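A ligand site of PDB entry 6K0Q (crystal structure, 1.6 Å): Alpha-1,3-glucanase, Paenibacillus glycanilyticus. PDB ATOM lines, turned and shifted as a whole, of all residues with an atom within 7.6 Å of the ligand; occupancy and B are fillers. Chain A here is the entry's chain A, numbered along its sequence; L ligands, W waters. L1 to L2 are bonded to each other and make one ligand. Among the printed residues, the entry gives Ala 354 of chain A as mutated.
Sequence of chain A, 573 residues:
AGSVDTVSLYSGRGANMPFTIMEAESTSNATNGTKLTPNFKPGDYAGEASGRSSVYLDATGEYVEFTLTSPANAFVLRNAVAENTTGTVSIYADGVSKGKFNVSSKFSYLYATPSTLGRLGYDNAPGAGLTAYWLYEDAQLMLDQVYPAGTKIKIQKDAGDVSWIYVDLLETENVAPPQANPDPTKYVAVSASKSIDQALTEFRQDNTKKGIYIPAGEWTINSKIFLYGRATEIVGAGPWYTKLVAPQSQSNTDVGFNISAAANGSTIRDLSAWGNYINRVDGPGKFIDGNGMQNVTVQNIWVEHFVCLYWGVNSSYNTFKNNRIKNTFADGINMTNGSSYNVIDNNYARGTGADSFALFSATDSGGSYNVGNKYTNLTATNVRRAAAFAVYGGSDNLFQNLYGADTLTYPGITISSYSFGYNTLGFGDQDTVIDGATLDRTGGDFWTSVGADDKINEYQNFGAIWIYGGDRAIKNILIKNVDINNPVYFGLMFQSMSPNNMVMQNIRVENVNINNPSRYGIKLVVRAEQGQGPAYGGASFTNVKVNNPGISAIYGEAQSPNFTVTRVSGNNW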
ATOM      1  N   TYR A 122     -19.835  -2.895 -17.884  1.00  0.00           N
ATOM      2  CA  TYR A 122     -19.067  -3.527 -18.950  1.00  0.00           C
ATOM      3  C   TYR A 122     -19.498  -4.946 -19.272  1.00  0.00           C
ATOM      4  O   TYR A 122     -19.275  -5.411 -20.395  1.00  0.00           O
ATOM      5  CB  TYR A 122     -17.583  -3.566 -18.562  1.00  0.00           C
ATOM      6  CG  TYR A 122     -16.859  -2.247 -18.652  1.00  0.00           C
ATOM      7  CD1 TYR A 122     -16.326  -1.806 -19.852  1.00  0.00           C
ATOM      8  CD2 TYR A 122     -16.665  -1.457 -17.512  1.00  0.00           C
ATOM      9  CE1 TYR A 122     -15.656  -0.611 -19.939  1.00  0.00           C
ATOM     10  CE2 TYR A 122     -15.984  -0.253 -17.597  1.00  0.00           C
ATOM     11  CZ  TYR A 122     -15.485   0.165 -18.812  1.00  0.00           C
ATOM     12  OH  TYR A 122     -14.799   1.350 -18.886  1.00  0.00           O
ATOM     13  N   ARG A 280     -21.166  -1.393 -21.851  1.00  0.00           N
ATOM     14  CA  ARG A 280     -20.237  -0.318 -22.172  1.00  0.00           C
ATOM     15  C   ARG A 280     -19.083  -0.847 -23.006  1.00  0.00           C
ATOM     16  O   ARG A 280     -18.577  -1.951 -22.756  1.00  0.00           O
ATOM     17  CB  ARG A 280     -19.721   0.313 -20.876  1.00  0.00           C
ATOM     18  CG  ARG A 280     -18.728   1.440 -21.054  1.00  0.00           C
ATOM     19  CD  ARG A 280     -18.370   2.018 -19.705  1.00  0.00           C
ATOM     20  NE  ARG A 280     -17.291   2.996 -19.794  1.00  0.00           N
ATOM     21  CZ  ARG A 280     -16.918   3.788 -18.803  1.00  0.00           C
ATOM     22  NH1 ARG A 280     -17.539   3.739 -17.633  1.00  0.00           N
ATOM     23  NH2 ARG A 280     -15.913   4.633 -18.972  1.00  0.00           N
ATOM     24  N   VAL A 281     -18.685  -0.063 -23.998  1.00  0.00           N
ATOM     25  CA  VAL A 281     -17.494  -0.287 -24.807  1.00  0.00           C
ATOM     26  C   VAL A 281     -16.791   1.050 -24.929  1.00  0.00           C
ATOM     27  O   VAL A 281     -17.438   2.075 -25.182  1.00  0.00           O
ATOM     28  CB  VAL A 281     -17.822  -0.865 -26.201  1.00  0.00           C
ATOM     29  CG1 VAL A 281     -16.557  -1.177 -26.989  1.00  0.00           C
ATOM     30  CG2 VAL A 281     -18.699  -2.117 -26.085  1.00  0.00           C
ATOM     31  N   ASP A 282     -15.472   1.078 -24.715  1.00  0.00           N
ATOM     32  CA  ASP A 282     -14.726   2.325 -24.663  1.00  0.00           C
ATOM     33  C   ASP A 282     -14.064   2.577 -26.013  1.00  0.00           C
ATOM     34  O   ASP A 282     -13.170   1.835 -26.437  1.00  0.00           O
ATOM     35  CB  ASP A 282     -13.708   2.301 -23.523  1.00  0.00           C
ATOM     36  CG  ASP A 282     -14.375   2.308 -22.161  1.00  0.00           C
ATOM     37  OD1 ASP A 282     -15.512   2.812 -22.056  1.00  0.00           O
ATOM     38  OD2 ASP A 282     -13.764   1.817 -21.197  1.00  0.00           O
ATOM     39  N   GLY A 283     -14.502   3.645 -26.678  1.00  0.00           N
ATOM     40  CA  GLY A 283     -14.068   3.973 -28.010  1.00  0.00           C
ATOM     41  C   GLY A 283     -15.264   4.267 -28.888  1.00  0.00           C
ATOM     42  O   GLY A 283     -15.689   5.418 -29.051  1.00  0.00           O
ATOM     43  N   PRO A 284     -15.867   3.214 -29.446  1.00  0.00           N
ATOM     44  CA  PRO A 284     -17.128   3.381 -30.174  1.00  0.00           C
ATOM     45  C   PRO A 284     -18.283   3.624 -29.221  1.00  0.00           C
ATOM     46  O   PRO A 284     -18.160   3.521 -27.999  1.00  0.00           O
ATOM     47  CB  PRO A 284     -17.287   2.039 -30.895  1.00  0.00           C
ATOM     48  CG  PRO A 284     -16.629   1.054 -29.961  1.00  0.00           C
ATOM     49  CD  PRO A 284     -15.475   1.798 -29.321  1.00  0.00           C
ATOM     50  N   GLY A 285     -19.423   3.981 -29.791  1.00  0.00           N
ATOM     51  CA  GLY A 285     -20.673   3.983 -29.071  1.00  0.00           C
ATOM     52  C   GLY A 285     -21.297   5.330 -28.757  1.00  0.00           C
ATOM     53  O   GLY A 285     -22.289   5.377 -28.029  1.00  0.00           O
ATOM     54  N   LYS A 286     -20.772   6.418 -29.307  1.00  0.00           N
ATOM     55  CA  LYS A 286     -21.412   7.716 -29.149  1.00  0.00           C
ATOM     56  C   LYS A 286     -22.401   7.921 -30.287  1.00  0.00           C
ATOM     57  O   LYS A 286     -22.051   7.699 -31.450  1.00  0.00           O
ATOM     58  CB  LYS A 286     -20.385   8.849 -29.118  1.00  0.00           C
ATOM     59  CG  LYS A 286     -19.497   8.847 -27.877  1.00  0.00           C
ATOM     60  CD  LYS A 286     -18.174   8.112 -28.128  1.00  0.00           C
ATOM     61  CE  LYS A 286     -17.209   8.275 -26.945  1.00  0.00           C
ATOM     62  NZ  LYS A 286     -15.894   7.594 -27.209  1.00  0.00           N
ATOM     63  N   ASN A 291     -15.706  15.327 -33.543  1.00  0.00           N
ATOM     64  CA  ASN A 291     -14.464  15.843 -32.982  1.00  0.00           C
ATOM     65  C   ASN A 291     -14.166  17.214 -33.572  1.00  0.00           C
ATOM     66  O   ASN A 291     -14.127  17.393 -34.787  1.00  0.00           O
ATOM     67  CB  ASN A 291     -13.318  14.872 -33.258  1.00  0.00           C
ATOM     68  CG  ASN A 291     -13.318  13.673 -32.321  1.00  0.00           C
ATOM     69  OD1 ASN A 291     -14.274  13.468 -31.561  1.00  0.00           O
ATOM     70  ND2 ASN A 291     -12.252  12.884 -32.380  1.00  0.00           N
ATOM     71  N   VAL A 307     -23.418   4.227 -25.781  1.00  0.00           N
ATOM     72  CA  VAL A 307     -22.469   4.500 -24.708  1.00  0.00           C
ATOM     73  C   VAL A 307     -22.611   5.946 -24.231  1.00  0.00           C
ATOM     74  O   VAL A 307     -22.727   6.209 -23.031  1.00  0.00           O
ATOM     75  CB  VAL A 307     -21.030   4.157 -25.159  1.00  0.00           C
ATOM     76  CG1 VAL A 307     -20.036   4.420 -24.035  1.00  0.00           C
ATOM     77  CG2 VAL A 307     -20.975   2.685 -25.578  1.00  0.00           C
ATOM     78  N   CYS A 308     -22.669   6.892 -25.180  1.00  0.00           N
ATOM     79  CA  CYS A 308     -22.872   8.310 -24.868  1.00  0.00           C
ATOM     80  C   CYS A 308     -23.808   8.918 -25.892  1.00  0.00           C
ATOM     81  O   CYS A 308     -23.945   8.412 -27.014  1.00  0.00           O
ATOM     82  CB  CYS A 308     -21.539   9.091 -24.910  1.00  0.00           C
ATOM     83  SG  CYS A 308     -20.233   8.444 -23.830  1.00  0.00           S
ATOM     84  N   TRP A 311     -19.508  13.051 -26.999  1.00  0.00           N
ATOM     85  CA  TRP A 311     -18.226  13.163 -26.279  1.00  0.00           C
ATOM     86  C   TRP A 311     -17.373  14.150 -27.063  1.00  0.00           C
ATOM     87  O   TRP A 311     -16.673  13.766 -28.008  1.00  0.00           O
ATOM     88  CB  TRP A 311     -17.580  11.789 -26.161  1.00  0.00           C
ATOM     89  CG  TRP A 311     -16.291  11.758 -25.372  1.00  0.00           C
ATOM     90  CD1 TRP A 311     -15.069  12.247 -25.757  1.00  0.00           C
ATOM     91  CD2 TRP A 311     -16.093  11.168 -24.075  1.00  0.00           C
ATOM     92  NE1 TRP A 311     -14.130  12.010 -24.779  1.00  0.00           N
ATOM     93  CE2 TRP A 311     -14.731  11.351 -23.735  1.00  0.00           C
ATOM     94  CE3 TRP A 311     -16.939  10.507 -23.174  1.00  0.00           C
ATOM     95  CZ2 TRP A 311     -14.205  10.893 -22.533  1.00  0.00           C
ATOM     96  CZ3 TRP A 311     -16.415  10.062 -21.976  1.00  0.00           C
ATOM     97  CH2 TRP A 311     -15.051  10.252 -21.668  1.00  0.00           C
ATOM     98  N   GLY A 312     -17.432  15.422 -26.677  1.00  0.00           N
ATOM     99  CA  GLY A 312     -16.762  16.464 -27.431  1.00  0.00           C
ATOM    100  C   GLY A 312     -15.264  16.465 -27.216  1.00  0.00           C
ATOM    101  O   GLY A 312     -14.758  16.136 -26.136  1.00  0.00           O
ATOM    102  N   VAL A 313     -14.532  16.814 -28.279  1.00  0.00           N
ATOM    103  CA  VAL A 313     -13.078  16.916 -28.279  1.00  0.00           C
ATOM    104  C   VAL A 313     -12.724  18.222 -28.985  1.00  0.00           C
ATOM    105  O   VAL A 313     -12.805  18.301 -30.211  1.00  0.00           O
ATOM    106  CB  VAL A 313     -12.403  15.729 -28.983  1.00  0.00           C
ATOM    107  CG1 VAL A 313     -10.894  15.864 -28.884  1.00  0.00           C
ATOM    108  CG2 VAL A 313     -12.889  14.415 -28.385  1.00  0.00           C
ATOM    109  N   PHE A 329     -24.624   3.658 -21.435  1.00  0.00           N
ATOM    110  CA  PHE A 329     -23.670   2.787 -20.765  1.00  0.00           C
ATOM    111  C   PHE A 329     -22.432   3.519 -20.278  1.00  0.00           C
ATOM    112  O   PHE A 329     -21.643   2.948 -19.524  1.00  0.00           O
ATOM    113  CB  PHE A 329     -23.348   1.591 -21.667  1.00  0.00           C
ATOM    114  CG  PHE A 329     -24.514   0.662 -21.775  1.00  0.00           C
ATOM    115  CD1 PHE A 329     -25.489   0.852 -22.746  1.00  0.00           C
ATOM    116  CD2 PHE A 329     -24.720  -0.325 -20.817  1.00  0.00           C
ATOM    117  CE1 PHE A 329     -26.607   0.038 -22.800  1.00  0.00           C
ATOM    118  CE2 PHE A 329     -25.845  -1.135 -20.856  1.00  0.00           C
ATOM    119  CZ  PHE A 329     -26.783  -0.960 -21.847  1.00  0.00           C
ATOM    120  N   ALA A 330     -22.269   4.792 -20.657  1.00  0.00           N
ATOM    121  CA  ALA A 330     -21.313   5.672 -19.985  1.00  0.00           C
ATOM    122  C   ALA A 330     -21.899   7.088 -19.942  1.00  0.00           C
ATOM    123  O   ALA A 330     -23.106   7.233 -19.763  1.00  0.00           O
ATOM    124  CB  ALA A 330     -19.928   5.652 -20.673  1.00  0.00           C
ATOM    125  N   ASP A 331     -21.052   8.109 -20.114  1.00  0.00           N
ATOM    126  CA  ASP A 331     -21.477   9.498 -19.944  1.00  0.00           C
ATOM    127  C   ASP A 331     -22.662   9.847 -20.841  1.00  0.00           C
ATOM    128  O   ASP A 331     -22.813   9.330 -21.941  1.00  0.00           O
ATOM    129  CB  ASP A 331     -20.344  10.484 -20.297  1.00  0.00           C
ATOM    130  CG  ASP A 331     -19.114  10.302 -19.459  1.00  0.00           C
ATOM    131  OD1 ASP A 331     -18.687   9.146 -19.288  1.00  0.00           O
ATOM    132  OD2 ASP A 331     -18.543  11.335 -19.023  1.00  0.00           O
ATOM    133  N   ASN A 334     -20.295  14.622 -22.503  1.00  0.00           N
ATOM    134  CA  ASN A 334     -18.996  15.054 -21.984  1.00  0.00           C
ATOM    135  C   ASN A 334     -18.380  15.990 -23.012  1.00  0.00           C
ATOM    136  O   ASN A 334     -18.539  15.777 -24.219  1.00  0.00           O
ATOM    137  CB  ASN A 334     -18.086  13.854 -21.722  1.00  0.00           C
ATOM    138  CG  ASN A 334     -16.859  14.197 -20.874  1.00  0.00           C
ATOM    139  OD1 ASN A 334     -16.682  15.328 -20.415  1.00  0.00           O
ATOM    140  ND2 ASN A 334     -15.999  13.196 -20.671  1.00  0.00           N
ATOM    141  N   THR A 336     -14.633  17.703 -23.795  1.00  0.00           N
ATOM    142  CA  THR A 336     -13.265  17.519 -23.337  1.00  0.00           C
ATOM    143  C   THR A 336     -12.280  18.332 -24.179  1.00  0.00           C
ATOM    144  O   THR A 336     -12.609  18.858 -25.245  1.00  0.00           O
ATOM    145  CB  THR A 336     -12.838  16.039 -23.369  1.00  0.00           C
ATOM    146  OG1 THR A 336     -12.471  15.674 -24.707  1.00  0.00           O
ATOM    147  CG2 THR A 336     -13.959  15.121 -22.872  1.00  0.00           C
ATOM    148  N   ASN A 337     -11.060  18.423 -23.658  1.00  0.00           N
ATOM    149  CA  ASN A 337      -9.866  18.762 -24.423  1.00  0.00           C
ATOM    150  C   ASN A 337     -10.027  20.034 -25.244  1.00  0.00           C
ATOM    151  O   ASN A 337      -9.831  20.051 -26.459  1.00  0.00           O
ATOM    152  CB  ASN A 337      -9.474  17.587 -25.333  1.00  0.00           C
ATOM    153  CG  ASN A 337      -9.127  16.331 -24.548  1.00  0.00           C
ATOM    154  OD1 ASN A 337      -9.362  16.264 -23.339  1.00  0.00           O
ATOM    155  ND2 ASN A 337      -8.564  15.348 -25.230  1.00  0.00           N
ATOM    156  N   ALA A 354     -22.229   6.481 -16.608  1.00  0.00           N
ATOM    157  CA  ALA A 354     -21.102   7.208 -15.995  1.00  0.00           C
ATOM    158  C   ALA A 354     -21.583   8.646 -15.863  1.00  0.00           C
ATOM    159  O   ALA A 354     -22.800   8.897 -15.931  1.00  0.00           O
ATOM    160  CB  ALA A 354     -19.816   7.044 -16.821  1.00  0.00           C
ATOM    161  N   PHE A 360     -14.452  17.898 -19.062  1.00  0.00           N
ATOM    162  CA  PHE A 360     -13.083  17.490 -18.737  1.00  0.00           C
ATOM    163  C   PHE A 360     -12.116  18.411 -19.462  1.00  0.00           C
ATOM    164  O   PHE A 360     -11.966  18.340 -20.679  1.00  0.00           O
ATOM    165  CB  PHE A 360     -12.794  16.030 -19.088  1.00  0.00           C
ATOM    166  CG  PHE A 360     -11.489  15.525 -18.524  1.00  0.00           C
ATOM    167  CD1 PHE A 360     -10.279  15.835 -19.119  1.00  0.00           C
ATOM    168  CD2 PHE A 360     -11.482  14.774 -17.361  1.00  0.00           C
ATOM    169  CE1 PHE A 360      -9.079  15.399 -18.579  1.00  0.00           C
ATOM    170  CE2 PHE A 360     -10.290  14.323 -16.815  1.00  0.00           C
ATOM    171  CZ  PHE A 360      -9.092  14.629 -17.421  1.00  0.00           C
ATOM    172  N   ALA A 362      -8.533  19.896 -20.533  1.00  0.00           N
ATOM    173  CA  ALA A 362      -7.197  19.394 -20.830  1.00  0.00           C
ATOM    174  C   ALA A 362      -6.641  20.198 -22.002  1.00  0.00           C
ATOM    175  O   ALA A 362      -7.372  20.894 -22.701  1.00  0.00           O
ATOM    176  CB  ALA A 362      -7.207  17.893 -21.149  1.00  0.00           C
ATOM    177  N   TYR A 422      -3.759  12.457 -18.018  1.00  0.00           N
ATOM    178  CA  TYR A 422      -3.771  13.287 -19.217  1.00  0.00           C
ATOM    179  C   TYR A 422      -3.028  14.592 -18.961  1.00  0.00           C
ATOM    180  O   TYR A 422      -2.627  14.900 -17.833  1.00  0.00           O
ATOM    181  CB  TYR A 422      -5.203  13.530 -19.668  1.00  0.00           C
ATOM    182  CG  TYR A 422      -5.959  12.258 -19.961  1.00  0.00           C
ATOM    183  CD1 TYR A 422      -5.669  11.511 -21.103  1.00  0.00           C
ATOM    184  CD2 TYR A 422      -6.939  11.776 -19.093  1.00  0.00           C
ATOM    185  CE1 TYR A 422      -6.345  10.342 -21.383  1.00  0.00           C
ATOM    186  CE2 TYR A 422      -7.614  10.592 -19.370  1.00  0.00           C
ATOM    187  CZ  TYR A 422      -7.318   9.882 -20.517  1.00  0.00           C
ATOM    188  OH  TYR A 422      -7.975   8.713 -20.802  1.00  0.00           O
HETATM  189  C1  LIG L   1     -13.223   5.960 -21.305  1.00  0.00           C
HETATM  190  C2  LIG L   1     -12.425   6.332 -22.542  1.00  0.00           C
HETATM  191  C3  LIG L   1     -13.167   7.367 -23.349  1.00  0.00           C
HETATM  192  C4  LIG L   1     -14.571   6.879 -23.652  1.00  0.00           C
HETATM  193  C5  LIG L   1     -15.267   6.624 -22.353  1.00  0.00           C
HETATM  194  C6  LIG L   1     -16.670   6.095 -22.584  1.00  0.00           C
HETATM  195  O1  LIG L   1     -13.197   7.032 -20.415  1.00  0.00           O
HETATM  196  O2  LIG L   1     -11.197   6.834 -22.116  1.00  0.00           O
HETATM  197  O3  LIG L   1     -12.581   7.433 -24.606  1.00  0.00           O
HETATM  198  O4  LIG L   1     -15.327   7.813 -24.382  1.00  0.00           O
HETATM  199  O5  LIG L   1     -14.540   5.646 -21.664  1.00  0.00           O
HETATM  200  O6  LIG L   1     -16.690   4.887 -23.256  1.00  0.00           O
HETATM  201  C1  LG2 L   2     -12.395   8.809 -25.027  1.00  0.00           C
HETATM  202  C2  LG2 L   2     -11.844   8.773 -26.442  1.00  0.00           C
HETATM  203  C3  LG2 L   2     -10.353   8.464 -26.372  1.00  0.00           C
HETATM  204  C4  LG2 L   2      -9.649   9.482 -25.481  1.00  0.00           C
HETATM  205  C5  LG2 L   2     -10.341   9.537 -24.120  1.00  0.00           C
HETATM  206  C6  LG2 L   2      -9.714  10.560 -23.166  1.00  0.00           C
HETATM  207  O1  LG2 L   2     -12.540   7.801 -27.212  1.00  0.00           O
HETATM  208  O2  LG2 L   2      -9.785   8.465 -27.674  1.00  0.00           O
HETATM  209  O3  LG2 L   2      -8.290   9.141 -25.294  1.00  0.00           O
HETATM  210  O4  LG2 L   2     -11.722   9.814 -24.291  1.00  0.00           O
HETATM  211  O5  LG2 L   2      -9.724  11.854 -23.720  1.00  0.00           O
HETATM  212  O   HOH W   1     -16.854   5.024 -25.996  1.00  0.00           O
HETATM  213  O   HOH W   2      -7.453   7.025 -23.041  1.00  0.00           O
HETATM  214  O   HOH W   3     -11.085   8.950 -20.071  1.00  0.00           O
HETATM  215  O   HOH W   4     -11.540  13.184 -25.141  1.00  0.00           O
HETATM  216  O   HOH W   5     -11.467   5.159 -26.603  1.00  0.00           O
HETATM  217  O   HOH W   6      -9.532   5.873 -28.503  1.00  0.00           O
HETATM  218  O   HOH W   7      -6.628  11.811 -25.197  1.00  0.00           O
HETATM  219  O   HOH W   8     -12.419   8.270 -29.927  1.00  0.00           O
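OD1 of Asp 282 is in hydrogen-bond range of O6 of LIG L1, at 2.7 Å. The side-chain amino group (NZ) of Lys 286 is in hydrogen-bond range of an oxygen (O4) of LIG L1, at 2.9 Å. The guanidinium group (NH2) of Arg 280 lies within hydrogen-bond range of an oxygen (O5) of LIG L1, at 3.2 Å. O4 of LG2 L2 lies close to NE1 of Trp 311, 3.3 Å away. The backbone carbonyl oxygen (O) of Val 281 sits at hydrogen-bond distance from an oxygen (O6) of LIG L1 (3.5 Å).
Merely in contact with the ligand: Val 307 (3.5 Å), Tyr 422 (3.5 Å), Ala 330 (3.8 Å) and Asn 337 (3.98 Å). Hydrophobic or aromatic side chains that line the ligand: Val 307, Trp 311, Ala 330 and Tyr 422. Along chain A the residues within 4 Å of the ligand span positions 280 to 422. The nearest printed residue that does not touch the ligand is Gly 283 (4.2 Å).
N of Asn 337 lies within hydrogen-bond range of O of Phe 360, 3.1 Å away. The side-chain hydroxyl (OH) of Tyr 122 sits at hydrogen-bond distance from the guanidinium group (NE) of Arg 280, at 3.1 Å. The backbone carbonyl oxygen (O) of Ala 330 lies within hydrogen-bond range of the backbone NH (N) of Ala 354 (3.4 Å). O of Val 307 is in hydrogen-bond range of N of Ala 330 (2.8 Å). The guanidinium group (NE) of Arg 280 is in salt-bridge range of the side-chain carboxylate (OD1) of Asp 282, at 2.9 Å. The backbone NH of Val 307 sits at hydrogen-bond distance from the backbone carbonyl oxygen of Gly 285 (2.8 Å). OH of Tyr 122 sits at hydrogen-bond distance from OD2 of Asp 282. The side-chain amide oxygen (OD1) of Asn 337 lies close to the side-chain hydroxyl (OG1) of Thr 336, at 3.4 Å.
Water W4 lies within hydrogen-bond range of O5 of LG2 L2, OG1 of Thr 336 and NE1 of Trp 311. Water W1 lies within hydrogen-bond range of O6 of LIG L1, N of Gly 283, O of Pro 284, NZ of Lys 286 and O of Val 281. Water W3 lies within hydrogen-bond range of an oxygen (O1) of LIG L1 (2.9 Å) and the side-chain hydroxyl (OH) of Tyr 422 (3.2 Å). Water W5 bridges an oxygen (O1) of LG2 L2 (2.9 Å) and the backbone NH (N) of Gly 283 (3.4 Å). Water W2 lies within hydrogen-bond range of the side-chain hydroxyl of Tyr 422 and an oxygen (O3) of LG2 L2.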
